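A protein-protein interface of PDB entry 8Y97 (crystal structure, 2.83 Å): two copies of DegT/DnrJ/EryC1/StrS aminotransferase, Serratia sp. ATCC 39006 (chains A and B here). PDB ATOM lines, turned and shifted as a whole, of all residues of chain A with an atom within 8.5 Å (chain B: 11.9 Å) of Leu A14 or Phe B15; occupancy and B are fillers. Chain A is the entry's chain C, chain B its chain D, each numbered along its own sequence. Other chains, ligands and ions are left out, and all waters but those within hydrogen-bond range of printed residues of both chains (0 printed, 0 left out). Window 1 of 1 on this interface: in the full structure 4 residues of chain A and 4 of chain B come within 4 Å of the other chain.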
ATOM      1  N   GLU A  12     -25.891 -16.990   9.713  1.00  0.00           N
ATOM      2  CA  GLU A  12     -25.519 -16.427  11.040  1.00  0.00           C
ATOM      3  C   GLU A  12     -26.553 -16.812  12.098  1.00  0.00           C
ATOM      4  O   GLU A  12     -26.231 -16.859  13.285  1.00  0.00           O
ATOM      5  CB  GLU A  12     -25.389 -14.905  10.949  1.00  0.00           C
ATOM      6  N   GLN A  13     -27.803 -17.030  11.666  1.00  0.00           N
ATOM      7  CA  GLN A  13     -28.881 -17.418  12.560  1.00  0.00           C
ATOM      8  C   GLN A  13     -28.613 -18.815  13.118  1.00  0.00           C
ATOM      9  O   GLN A  13     -28.757 -19.039  14.317  1.00  0.00           O
ATOM     10  CB  GLN A  13     -30.217 -17.385  11.817  1.00  0.00           C
ATOM     11  CG  GLN A  13     -31.439 -17.384  12.729  1.00  0.00           C
ATOM     12  CD  GLN A  13     -32.717 -17.704  11.985  1.00  0.00           C
ATOM     13  OE1 GLN A  13     -32.858 -18.782  11.396  1.00  0.00           O
ATOM     14  NE2 GLN A  13     -33.661 -16.772  11.995  1.00  0.00           N
ATOM     15  N   LEU A  14     -28.221 -19.744  12.237  1.00  0.00           N
ATOM     16  CA  LEU A  14     -28.016 -21.132  12.620  1.00  0.00           C
ATOM     17  C   LEU A  14     -26.936 -21.234  13.696  1.00  0.00           C
ATOM     18  O   LEU A  14     -27.027 -22.088  14.575  1.00  0.00           O
ATOM     19  CB  LEU A  14     -27.667 -21.974  11.394  1.00  0.00           C
ATOM     20  CG  LEU A  14     -28.788 -22.162  10.364  1.00  0.00           C
ATOM     21  CD1 LEU A  14     -28.256 -22.881   9.136  1.00  0.00           C
ATOM     22  CD2 LEU A  14     -29.986 -22.915  10.930  1.00  0.00           C
ATOM     23  N   PHE A  15     -25.923 -20.362  13.629  1.00  0.00           N
ATOM     24  CA  PHE A  15     -24.845 -20.367  14.605  1.00  0.00           C
ATOM     25  C   PHE A  15     -25.351 -19.821  15.938  1.00  0.00           C
ATOM     26  O   PHE A  15     -25.125 -20.430  16.984  1.00  0.00           O
ATOM     27  CB  PHE A  15     -23.634 -19.568  14.110  1.00  0.00           C
ATOM     28  CG  PHE A  15     -22.516 -19.460  15.138  1.00  0.00           C
ATOM     29  CD1 PHE A  15     -21.709 -20.555  15.436  1.00  0.00           C
ATOM     30  CD2 PHE A  15     -22.276 -18.265  15.810  1.00  0.00           C
ATOM     31  CE1 PHE A  15     -20.696 -20.455  16.379  1.00  0.00           C
ATOM     32  CE2 PHE A  15     -21.257 -18.169  16.747  1.00  0.00           C
ATOM     33  CZ  PHE A  15     -20.471 -19.262  17.030  1.00  0.00           C
ATOM     34  N   GLN A  16     -26.027 -18.667  15.885  1.00  0.00           N
ATOM     35  CA  GLN A  16     -26.515 -17.988  17.076  1.00  0.00           C
ATOM     36  C   GLN A  16     -27.480 -18.889  17.846  1.00  0.00           C
ATOM     37  O   GLN A  16     -27.429 -18.935  19.075  1.00  0.00           O
ATOM     38  CB  GLN A  16     -27.156 -16.656  16.687  1.00  0.00           C
ATOM     39  CG  GLN A  16     -26.155 -15.601  16.227  1.00  0.00           C
ATOM     40  CD  GLN A  16     -26.793 -14.440  15.495  1.00  0.00           C
ATOM     41  OE1 GLN A  16     -28.008 -14.399  15.268  1.00  0.00           O
ATOM     42  NE2 GLN A  16     -25.969 -13.481  15.095  1.00  0.00           N
ATOM     43  N   VAL A  17     -28.351 -19.600  17.116  1.00  0.00           N
ATOM     44  CA  VAL A  17     -29.298 -20.529  17.715  1.00  0.00           C
ATOM     45  C   VAL A  17     -28.532 -21.685  18.352  1.00  0.00           C
ATOM     46  O   VAL A  17     -28.758 -22.011  19.515  1.00  0.00           O
ATOM     47  CB  VAL A  17     -30.329 -21.034  16.687  1.00  0.00           C
ATOM     48  CG1 VAL A  17     -31.177 -22.179  17.229  1.00  0.00           C
ATOM     49  CG2 VAL A  17     -31.227 -19.904  16.197  1.00  0.00           C
ATOM     50  N   SER A  18     -27.631 -22.296  17.576  1.00  0.00           N
ATOM     51  CA  SER A  18     -26.831 -23.417  18.045  1.00  0.00           C
ATOM     52  C   SER A  18     -26.026 -23.027  19.282  1.00  0.00           C
ATOM     53  O   SER A  18     -25.898 -23.819  20.215  1.00  0.00           O
ATOM     54  CB  SER A  18     -25.921 -23.936  16.951  1.00  0.00           C
ATOM     55  OG  SER A  18     -26.668 -24.461  15.864  1.00  0.00           O
ATOM     56  N   PHE A  19     -25.480 -21.805  19.278  1.00  0.00           N
ATOM     57  CA  PHE A  19     -24.599 -21.356  20.342  1.00  0.00           C
ATOM     58  C   PHE A  19     -25.373 -21.282  21.656  1.00  0.00           C
ATOM     59  O   PHE A  19     -24.871 -21.710  22.696  1.00  0.00           O
ATOM     60  CB  PHE A  19     -23.971 -20.001  19.994  1.00  0.00           C
ATOM     61  CG  PHE A  19     -23.016 -19.478  21.058  1.00  0.00           C
ATOM     62  CD1 PHE A  19     -23.490 -18.741  22.139  1.00  0.00           C
ATOM     63  CD2 PHE A  19     -21.652 -19.742  20.987  1.00  0.00           C
ATOM     64  CE1 PHE A  19     -22.621 -18.276  23.115  1.00  0.00           C
ATOM     65  CE2 PHE A  19     -20.788 -19.273  21.965  1.00  0.00           C
ATOM     66  CZ  PHE A  19     -21.272 -18.541  23.026  1.00  0.00           C
ATOM     67  N   VAL A  20     -26.593 -20.733  21.596  1.00  0.00           N
ATOM     68  CA  VAL A  20     -27.384 -20.517  22.795  1.00  0.00           C
ATOM     69  C   VAL A  20     -27.866 -21.866  23.333  1.00  0.00           C
ATOM     70  O   VAL A  20     -27.846 -22.086  24.544  1.00  0.00           O
ATOM     71  CB  VAL A  20     -28.520 -19.493  22.583  1.00  0.00           C
ATOM     72  CG1 VAL A  20     -29.615 -19.958  21.630  1.00  0.00           C
ATOM     73  CG2 VAL A  20     -29.129 -19.051  23.908  1.00  0.00           C
ATOM     74  N   LEU A  21     -28.263 -22.775  22.435  1.00  0.00           N
ATOM     75  CA  LEU A  21     -28.681 -24.112  22.827  1.00  0.00           C
ATOM     76  C   LEU A  21     -27.511 -24.863  23.457  1.00  0.00           C
ATOM     77  O   LEU A  21     -27.698 -25.598  24.422  1.00  0.00           O
ATOM     78  CB  LEU A  21     -29.238 -24.853  21.612  1.00  0.00           C
ATOM     79  CG  LEU A  21     -30.564 -24.320  21.060  1.00  0.00           C
ATOM     80  CD1 LEU A  21     -30.857 -24.922  19.697  1.00  0.00           C
ATOM     81  CD2 LEU A  21     -31.703 -24.607  22.023  1.00  0.00           C
ATOM     82  N   PHE A 142     -38.976 -21.484  17.216  1.00  0.00           N
ATOM     83  CA  PHE A 142     -38.270 -22.116  18.318  1.00  0.00           C
ATOM     84  C   PHE A 142     -39.221 -23.020  19.098  1.00  0.00           C
ATOM     85  O   PHE A 142     -38.821 -23.618  20.093  1.00  0.00           O
ATOM     86  CB  PHE A 142     -37.683 -21.034  19.228  1.00  0.00           C
ATOM     87  CG  PHE A 142     -36.645 -20.137  18.570  1.00  0.00           C
ATOM     88  CD1 PHE A 142     -35.589 -20.675  17.840  1.00  0.00           C
ATOM     89  CD2 PHE A 142     -36.734 -18.753  18.677  1.00  0.00           C
ATOM     90  CE1 PHE A 142     -34.642 -19.851  17.252  1.00  0.00           C
ATOM     91  CE2 PHE A 142     -35.789 -17.934  18.079  1.00  0.00           C
ATOM     92  CZ  PHE A 142     -34.746 -18.482  17.367  1.00  0.00           C
ATOM     93  N   MET A 203     -32.395 -14.628  23.127  1.00  0.00           N
ATOM     94  CA  MET A 203     -31.287 -14.321  22.236  1.00  0.00           C
ATOM     95  C   MET A 203     -31.801 -13.520  21.041  1.00  0.00           C
ATOM     96  O   MET A 203     -31.263 -12.461  20.732  1.00  0.00           O
ATOM     97  CB  MET A 203     -30.594 -15.614  21.786  1.00  0.00           C
ATOM     98  CG  MET A 203     -29.480 -15.433  20.766  1.00  0.00           C
ATOM     99  SD  MET A 203     -30.038 -15.402  19.050  1.00  0.00           S
ATOM    100  CE  MET A 203     -30.761 -17.027  18.790  1.00  0.00           C
ATOM    101  N   GLU B  12     -23.019 -18.346   9.231  1.00  0.00           N
ATOM    102  CA  GLU B  12     -23.072 -19.210   8.020  1.00  0.00           C
ATOM    103  C   GLU B  12     -21.780 -20.020   7.944  1.00  0.00           C
ATOM    104  O   GLU B  12     -21.816 -21.246   7.994  1.00  0.00           O
ATOM    105  CB  GLU B  12     -23.308 -18.391   6.749  1.00  0.00           C
ATOM    106  N   GLN B  13     -20.641 -19.320   7.878  1.00  0.00           N
ATOM    107  CA  GLN B  13     -19.337 -19.956   7.996  1.00  0.00           C
ATOM    108  C   GLN B  13     -19.160 -20.507   9.408  1.00  0.00           C
ATOM    109  O   GLN B  13     -18.714 -21.638   9.578  1.00  0.00           O
ATOM    110  CB  GLN B  13     -18.183 -19.009   7.666  1.00  0.00           C
ATOM    111  CG  GLN B  13     -17.780 -19.012   6.195  1.00  0.00           C
ATOM    112  CD  GLN B  13     -16.362 -18.535   5.953  1.00  0.00           C
ATOM    113  OE1 GLN B  13     -15.562 -18.355   6.879  1.00  0.00           O
ATOM    114  NE2 GLN B  13     -16.030 -18.342   4.686  1.00  0.00           N
ATOM    115  N   LEU B  14     -19.524 -19.699  10.413  1.00  0.00           N
ATOM    116  CA  LEU B  14     -19.372 -20.063  11.813  1.00  0.00           C
ATOM    117  C   LEU B  14     -20.120 -21.361  12.114  1.00  0.00           C
ATOM    118  O   LEU B  14     -19.651 -22.173  12.908  1.00  0.00           O
ATOM    119  CB  LEU B  14     -19.873 -18.921  12.698  1.00  0.00           C
ATOM    120  CG  LEU B  14     -19.067 -17.620  12.652  1.00  0.00           C
ATOM    121  CD1 LEU B  14     -19.818 -16.493  13.339  1.00  0.00           C
ATOM    122  CD2 LEU B  14     -17.700 -17.819  13.281  1.00  0.00           C
ATOM    123  N   PHE B  15     -21.285 -21.544  11.482  1.00  0.00           N
ATOM    124  CA  PHE B  15     -22.096 -22.730  11.698  1.00  0.00           C
ATOM    125  C   PHE B  15     -21.440 -23.933  11.026  1.00  0.00           C
ATOM    126  O   PHE B  15     -21.297 -24.982  11.645  1.00  0.00           O
ATOM    127  CB  PHE B  15     -23.525 -22.524  11.188  1.00  0.00           C
ATOM    128  CG  PHE B  15     -24.392 -23.771  11.292  1.00  0.00           C
ATOM    129  CD1 PHE B  15     -24.869 -24.207  12.524  1.00  0.00           C
ATOM    130  CD2 PHE B  15     -24.724 -24.509  10.159  1.00  0.00           C
ATOM    131  CE1 PHE B  15     -25.655 -25.346  12.617  1.00  0.00           C
ATOM    132  CE2 PHE B  15     -25.511 -25.647  10.258  1.00  0.00           C
ATOM    133  CZ  PHE B  15     -25.973 -26.064  11.485  1.00  0.00           C
ATOM    134  N   GLN B  16     -21.052 -23.767   9.756  1.00  0.00           N
ATOM    135  CA  GLN B  16     -20.474 -24.843   8.963  1.00  0.00           C
ATOM    136  C   GLN B  16     -19.191 -25.359   9.615  1.00  0.00           C
ATOM    137  O   GLN B  16     -18.963 -26.565   9.643  1.00  0.00           O
ATOM    138  CB  GLN B  16     -20.254 -24.359   7.528  1.00  0.00           C
ATOM    139  CG  GLN B  16     -21.551 -24.190   6.742  1.00  0.00           C
ATOM    140  CD  GLN B  16     -21.402 -23.364   5.482  1.00  0.00           C
ATOM    141  OE1 GLN B  16     -20.315 -22.879   5.144  1.00  0.00           O
ATOM    142  NE2 GLN B  16     -22.505 -23.197   4.767  1.00  0.00           N
ATOM    143  N   VAL B  17     -18.369 -24.441  10.141  1.00  0.00           N
ATOM    144  CA  VAL B  17     -17.140 -24.800  10.833  1.00  0.00           C
ATOM    145  C   VAL B  17     -17.490 -25.554  12.114  1.00  0.00           C
ATOM    146  O   VAL B  17     -16.954 -26.629  12.375  1.00  0.00           O
ATOM    147  CB  VAL B  17     -16.272 -23.563  11.137  1.00  0.00           C
ATOM    148  CG1 VAL B  17     -15.103 -23.887  12.063  1.00  0.00           C
ATOM    149  CG2 VAL B  17     -15.767 -22.902   9.861  1.00  0.00           C
ATOM    150  N   SER B  18     -18.387 -24.970  12.915  1.00  0.00           N
ATOM    151  CA  SER B  18     -18.807 -25.564  14.175  1.00  0.00           C
ATOM    152  C   SER B  18     -19.406 -26.950  13.945  1.00  0.00           C
ATOM    153  O   SER B  18     -19.175 -27.862  14.733  1.00  0.00           O
ATOM    154  CB  SER B  18     -19.779 -24.664  14.901  1.00  0.00           C
ATOM    155  OG  SER B  18     -19.158 -23.439  15.272  1.00  0.00           O
ATOM    156  N   PHE B  19     -20.177 -27.098  12.864  1.00  0.00           N
ATOM    157  CA  PHE B  19     -20.884 -28.337  12.586  1.00  0.00           C
ATOM    158  C   PHE B  19     -19.881 -29.460  12.331  1.00  0.00           C
ATOM    159  O   PHE B  19     -20.053 -30.568  12.835  1.00  0.00           O
ATOM    160  CB  PHE B  19     -21.838 -28.170  11.399  1.00  0.00           C
ATOM    161  CG  PHE B  19     -22.655 -29.419  11.103  1.00  0.00           C
ATOM    162  CD1 PHE B  19     -23.852 -29.660  11.772  1.00  0.00           C
ATOM    163  CD2 PHE B  19     -22.221 -30.356  10.172  1.00  0.00           C
ATOM    164  CE1 PHE B  19     -24.592 -30.803  11.512  1.00  0.00           C
ATOM    165  CE2 PHE B  19     -22.964 -31.498   9.917  1.00  0.00           C
ATOM    166  CZ  PHE B  19     -24.147 -31.719  10.586  1.00  0.00           C
ATOM    167  N   VAL B  20     -18.842 -29.159  11.544  1.00  0.00           N
ATOM    168  CA  VAL B  20     -17.833 -30.136  11.163  1.00  0.00           C
ATOM    169  C   VAL B  20     -17.034 -30.553  12.394  1.00  0.00           C
ATOM    170  O   VAL B  20     -16.754 -31.734  12.582  1.00  0.00           O
ATOM    171  CB  VAL B  20     -16.910 -29.570  10.066  1.00  0.00           C
ATOM    172  CG1 VAL B  20     -15.484 -30.099  10.168  1.00  0.00           C
ATOM    173  CG2 VAL B  20     -17.490 -29.795   8.676  1.00  0.00           C
ATOM    174  N   LEU B  21     -16.654 -29.566  13.212  1.00  0.00           N
ATOM    175  CA  LEU B  21     -15.904 -29.819  14.432  1.00  0.00           C
ATOM    176  C   LEU B  21     -16.742 -30.661  15.393  1.00  0.00           C
ATOM    177  O   LEU B  21     -16.215 -31.547  16.058  1.00  0.00           O
ATOM    178  CB  LEU B  21     -15.477 -28.493  15.056  1.00  0.00           C
ATOM    179  CG  LEU B  21     -14.447 -27.686  14.258  1.00  0.00           C
ATOM    180  CD1 LEU B  21     -14.330 -26.269  14.796  1.00  0.00           C
ATOM    181  CD2 LEU B  21     -13.088 -28.367  14.265  1.00  0.00           C
ATOM    182  N   ALA B  22     -18.052 -30.389  15.445  1.00  0.00           N
ATOM    183  CA  ALA B  22     -18.964 -31.141  16.294  1.00  0.00           C
ATOM    184  C   ALA B  22     -19.083 -32.583  15.803  1.00  0.00           C
ATOM    185  O   ALA B  22     -19.062 -33.511  16.609  1.00  0.00           O
ATOM    186  CB  ALA B  22     -20.314 -30.458  16.337  1.00  0.00           C
ATOM    187  N   ARG B  23     -19.205 -32.757  14.479  1.00  0.00           N
ATOM    188  CA  ARG B  23     -19.385 -34.071  13.877  1.00  0.00           C
ATOM    189  C   ARG B  23     -18.188 -34.965  14.199  1.00  0.00           C
ATOM    190  O   ARG B  23     -18.364 -36.097  14.648  1.00  0.00           O
ATOM    191  CB  ARG B  23     -19.571 -33.973  12.357  1.00  0.00           C
ATOM    192  CG  ARG B  23     -19.804 -35.311  11.666  1.00  0.00           C
ATOM    193  CD  ARG B  23     -20.052 -35.191  10.168  1.00  0.00           C
ATOM    194  NE  ARG B  23     -18.949 -34.537   9.453  1.00  0.00           N
ATOM    195  CZ  ARG B  23     -17.718 -35.022   9.304  1.00  0.00           C
ATOM    196  NH1 ARG B  23     -17.400 -36.210   9.787  1.00  0.00           N
ATOM    197  NH2 ARG B  23     -16.803 -34.316   8.660  1.00  0.00           N
ATOM    198  N   VAL B  24     -16.979 -34.442  13.962  1.00  0.00           N
ATOM    199  CA  VAL B  24     -15.760 -35.212  14.151  1.00  0.00           C
ATOM    200  C   VAL B  24     -15.560 -35.479  15.643  1.00  0.00           C
ATOM    201  O   VAL B  24     -15.157 -36.575  16.021  1.00  0.00           O
ATOM    202  CB  VAL B  24     -14.538 -34.511  13.524  1.00  0.00           C
ATOM    203  CG1 VAL B  24     -13.235 -35.234  13.842  1.00  0.00           C
ATOM    204  CG2 VAL B  24     -14.690 -34.352  12.015  1.00  0.00           C
ATOM    205  N   LEU B  25     -15.848 -34.478  16.482  1.00  0.00           N
ATOM    206  CA  LEU B  25     -15.728 -34.637  17.925  1.00  0.00           C
ATOM    207  C   LEU B  25     -16.718 -35.694  18.413  1.00  0.00           C
ATOM    208  O   LEU B  25     -16.406 -36.456  19.327  1.00  0.00           O
ATOM    209  CB  LEU B  25     -15.932 -33.305  18.647  1.00  0.00           C
ATOM    210  CG  LEU B  25     -14.767 -32.313  18.568  1.00  0.00           C
ATOM    211  CD1 LEU B  25     -15.190 -30.958  19.105  1.00  0.00           C
ATOM    212  CD2 LEU B  25     -13.545 -32.819  19.315  1.00  0.00           C
ATOM    213  N   THR B  26     -17.905 -35.738  17.793  1.00  0.00           N
ATOM    214  CA  THR B  26     -18.912 -36.726  18.148  1.00  0.00           C
ATOM    215  C   THR B  26     -18.422 -38.118  17.751  1.00  0.00           C
ATOM    216  O   THR B  26     -18.679 -39.083  18.469  1.00  0.00           O
ATOM    217  CB  THR B  26     -20.249 -36.381  17.493  1.00  0.00           C
ATOM    218  OG1 THR B  26     -20.538 -35.048  17.901  1.00  0.00           O
ATOM    219  CG2 THR B  26     -21.373 -37.301  17.937  1.00  0.00           C
ATOM    220  N   TRP B 116      -9.547 -17.711   1.107  1.00  0.00           N
ATOM    221  CA  TRP B 116     -10.980 -17.741   0.853  1.00  0.00           C
ATOM    222  C   TRP B 116     -11.327 -17.052  -0.467  1.00  0.00           C
ATOM    223  O   TRP B 116     -12.390 -17.305  -1.032  1.00  0.00           O
ATOM    224  CB  TRP B 116     -11.737 -17.115   2.031  1.00  0.00           C
ATOM    225  CG  TRP B 116     -11.722 -17.978   3.265  1.00  0.00           C
ATOM    226  CD1 TRP B 116     -10.927 -17.845   4.367  1.00  0.00           C
ATOM    227  CD2 TRP B 116     -12.548 -19.138   3.503  1.00  0.00           C
ATOM    228  NE1 TRP B 116     -11.203 -18.835   5.273  1.00  0.00           N
ATOM    229  CE2 TRP B 116     -12.192 -19.640   4.774  1.00  0.00           C
ATOM    230  CE3 TRP B 116     -13.554 -19.787   2.778  1.00  0.00           C
ATOM    231  CZ2 TRP B 116     -12.809 -20.761   5.325  1.00  0.00           C
ATOM    232  CZ3 TRP B 116     -14.168 -20.891   3.330  1.00  0.00           C
ATOM    233  CH2 TRP B 116     -13.795 -21.374   4.584  1.00  0.00           C
ATOM    234  N   PHE B 142      -7.805 -22.226   9.789  1.00  0.00           N
ATOM    235  CA  PHE B 142      -8.098 -23.433  10.548  1.00  0.00           C
ATOM    236  C   PHE B 142      -6.827 -23.950  11.220  1.00  0.00           C
ATOM    237  O   PHE B 142      -6.858 -24.985  11.880  1.00  0.00           O
ATOM    238  CB  PHE B 142      -8.699 -24.499   9.626  1.00  0.00           C
ATOM    239  CG  PHE B 142     -10.021 -24.107   8.980  1.00  0.00           C
ATOM    240  CD1 PHE B 142     -11.068 -23.610   9.750  1.00  0.00           C
ATOM    241  CD2 PHE B 142     -10.208 -24.213   7.604  1.00  0.00           C
ATOM    242  CE1 PHE B 142     -12.268 -23.242   9.160  1.00  0.00           C
ATOM    243  CE2 PHE B 142     -11.411 -23.844   7.021  1.00  0.00           C
ATOM    244  CZ  PHE B 142     -12.437 -23.363   7.800  1.00  0.00           C
ATOM    245  N   LEU B 196      -9.206 -32.924  12.841  1.00  0.00           N
ATOM    246  CA  LEU B 196     -10.154 -31.837  13.017  1.00  0.00           C
ATOM    247  C   LEU B 196      -9.852 -30.721  12.019  1.00  0.00           C
ATOM    248  O   LEU B 196     -10.759 -30.224  11.358  1.00  0.00           O
ATOM    249  CB  LEU B 196     -10.124 -31.323  14.456  1.00  0.00           C
ATOM    250  CG  LEU B 196     -10.839 -32.189  15.498  1.00  0.00           C
ATOM    251  CD1 LEU B 196     -10.477 -31.753  16.906  1.00  0.00           C
ATOM    252  CD2 LEU B 196     -12.342 -32.132  15.303  1.00  0.00           C
ATOM    253  N   ALA B 199     -10.630 -31.863   8.456  1.00  0.00           N
ATOM    254  CA  ALA B 199     -12.058 -31.923   8.174  1.00  0.00           C
ATOM    255  C   ALA B 199     -12.599 -30.538   7.822  1.00  0.00           C
ATOM    256  O   ALA B 199     -13.478 -30.411   6.974  1.00  0.00           O
ATOM    257  CB  ALA B 199     -12.793 -32.517   9.358  1.00  0.00           C
ATOM    258  N   CYS B 200     -12.073 -29.506   8.492  1.00  0.00           N
ATOM    259  CA  CYS B 200     -12.501 -28.135   8.264  1.00  0.00           C
ATOM    260  C   CYS B 200     -12.152 -27.707   6.843  1.00  0.00           C
ATOM    261  O   CYS B 200     -12.962 -27.069   6.170  1.00  0.00           O
ATOM    262  CB  CYS B 200     -11.892 -27.185   9.289  1.00  0.00           C
ATOM    263  SG  CYS B 200     -12.621 -27.355  10.940  1.00  0.00           S
ATOM    264  N   MET B 203     -14.294 -29.532   4.297  1.00  0.00           N
ATOM    265  CA  MET B 203     -15.597 -28.889   4.236  1.00  0.00           C
ATOM    266  C   MET B 203     -15.516 -27.644   3.355  1.00  0.00           C
ATOM    267  O   MET B 203     -16.318 -27.485   2.438  1.00  0.00           O
ATOM    268  CB  MET B 203     -16.087 -28.539   5.648  1.00  0.00           C
ATOM    269  CG  MET B 203     -17.399 -27.756   5.710  1.00  0.00           C
ATOM    270  SD  MET B 203     -17.225 -25.963   5.568  1.00  0.00           S
ATOM    271  CE  MET B 203     -16.275 -25.529   7.032  1.00  0.00           C
ATOM    272  N   ALA B 204     -14.537 -26.777   3.640  1.00  0.00           N
ATOM    273  CA  ALA B 204     -14.352 -25.533   2.908  1.00  0.00           C
ATOM    274  C   ALA B 204     -14.283 -25.795   1.402  1.00  0.00           C
ATOM    275  O   ALA B 204     -14.906 -25.083   0.615  1.00  0.00           O
ATOM    276  CB  ALA B 204     -13.107 -24.828   3.407  1.00  0.00           C
ATOM    277  N   LYS B 207     -17.705 -26.873  -0.069  1.00  0.00           N
ATOM    278  CA  LYS B 207     -18.670 -25.785  -0.139  1.00  0.00           C
ATOM    279  C   LYS B 207     -18.385 -24.904  -1.354  1.00  0.00           C
ATOM    280  O   LYS B 207     -19.310 -24.349  -1.941  1.00  0.00           O
ATOM    281  CB  LYS B 207     -18.665 -24.948   1.146  1.00  0.00           C
ATOM    282  CG  LYS B 207     -19.097 -25.678   2.412  1.00  0.00           C
ATOM    283  CD  LYS B 207     -20.506 -26.260   2.396  1.00  0.00           C
ATOM    284  CE  LYS B 207     -20.853 -26.930   3.690  1.00  0.00           C
ATOM    285  NZ  LYS B 207     -22.105 -27.685   3.598  1.00  0.00           N
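N of Glu B12 lies close to N of Glu A12 (3.2 Å).
O of Leu A14 sits at hydrogen-bond distance from OG of Ser A18, at 2.7 Å.
O of Leu B14 sits at hydrogen-bond distance from OG of Ser B18.
Among the printed residues, merely in contact across the chains: Ser A18 with Phe B15 (3.5 Å), Phe A15 with Ser B18 (3.5 Å), Phe A15 with Leu B14 (3.6 Å) and Leu A14 with Phe B15 (3.7 Å).
Leu A14 touches just one residue of chain B: Phe B15 (3.7 Å).
Phe B15 touches just these residues of chain A: Leu A14 (3.7 Å) and Ser A18 (3.5 Å).
Of chain B, only Leu B14 (3.6 Å) and Ser B18 (3.5 Å) come within 4 Å of Phe A15.
No residue of chain B comes within 4 Å of Gln A16.
No residue of chain B comes within 4 Å of Val A17.
Printed residues of chain A within 4 Å of Glu B12: Glu A12 (3.2 Å).
Of the printed residues of chain A, Leu B14 touches Phe A15.
Of the printed residues of chain A, Ser B18 touches Phe A15 (3.5 Å).
Lys B207 touches none of the printed residues of chain A.
Phe A142 touches none of the printed residues of chain B.
Hydrophobic or aromatic side chains of chain A within 4 Å of the printed part of chain B: Leu A14 and Phe A15.
Of the 23 printed residues of chain B, 4 touch a printed residue of chain A.
Printed residues of chain B that touch a printed residue of chain A: Glu B12, Leu B14, Phe B15 and Ser B18.
Hydrophobic or aromatic side chains of chain B that line the printed part of chain A: Leu B14 and Phe B15.
Among the printed residues, no Asp or Glu carboxylate lies within 4 Å of a Lys or Arg side-chain nitrogen of the other chain.
Glu B12 touches its own counterpart, Glu A12.
Leu A14 touches Phe B15, and with the chains exchanged Phe A15 touches Leu B14.
Phe A15 touches Ser B18, and with the chains exchanged Ser A18 touches Phe B15.
Positions printed for both chains: 12, 13, 14, 15, 16, 17, 18, 19, 20, 21, 142 and 203.
Of the 5 pairs that touch across the chains among the printed residues, 5 have their exchanged pair printed and touching as well.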
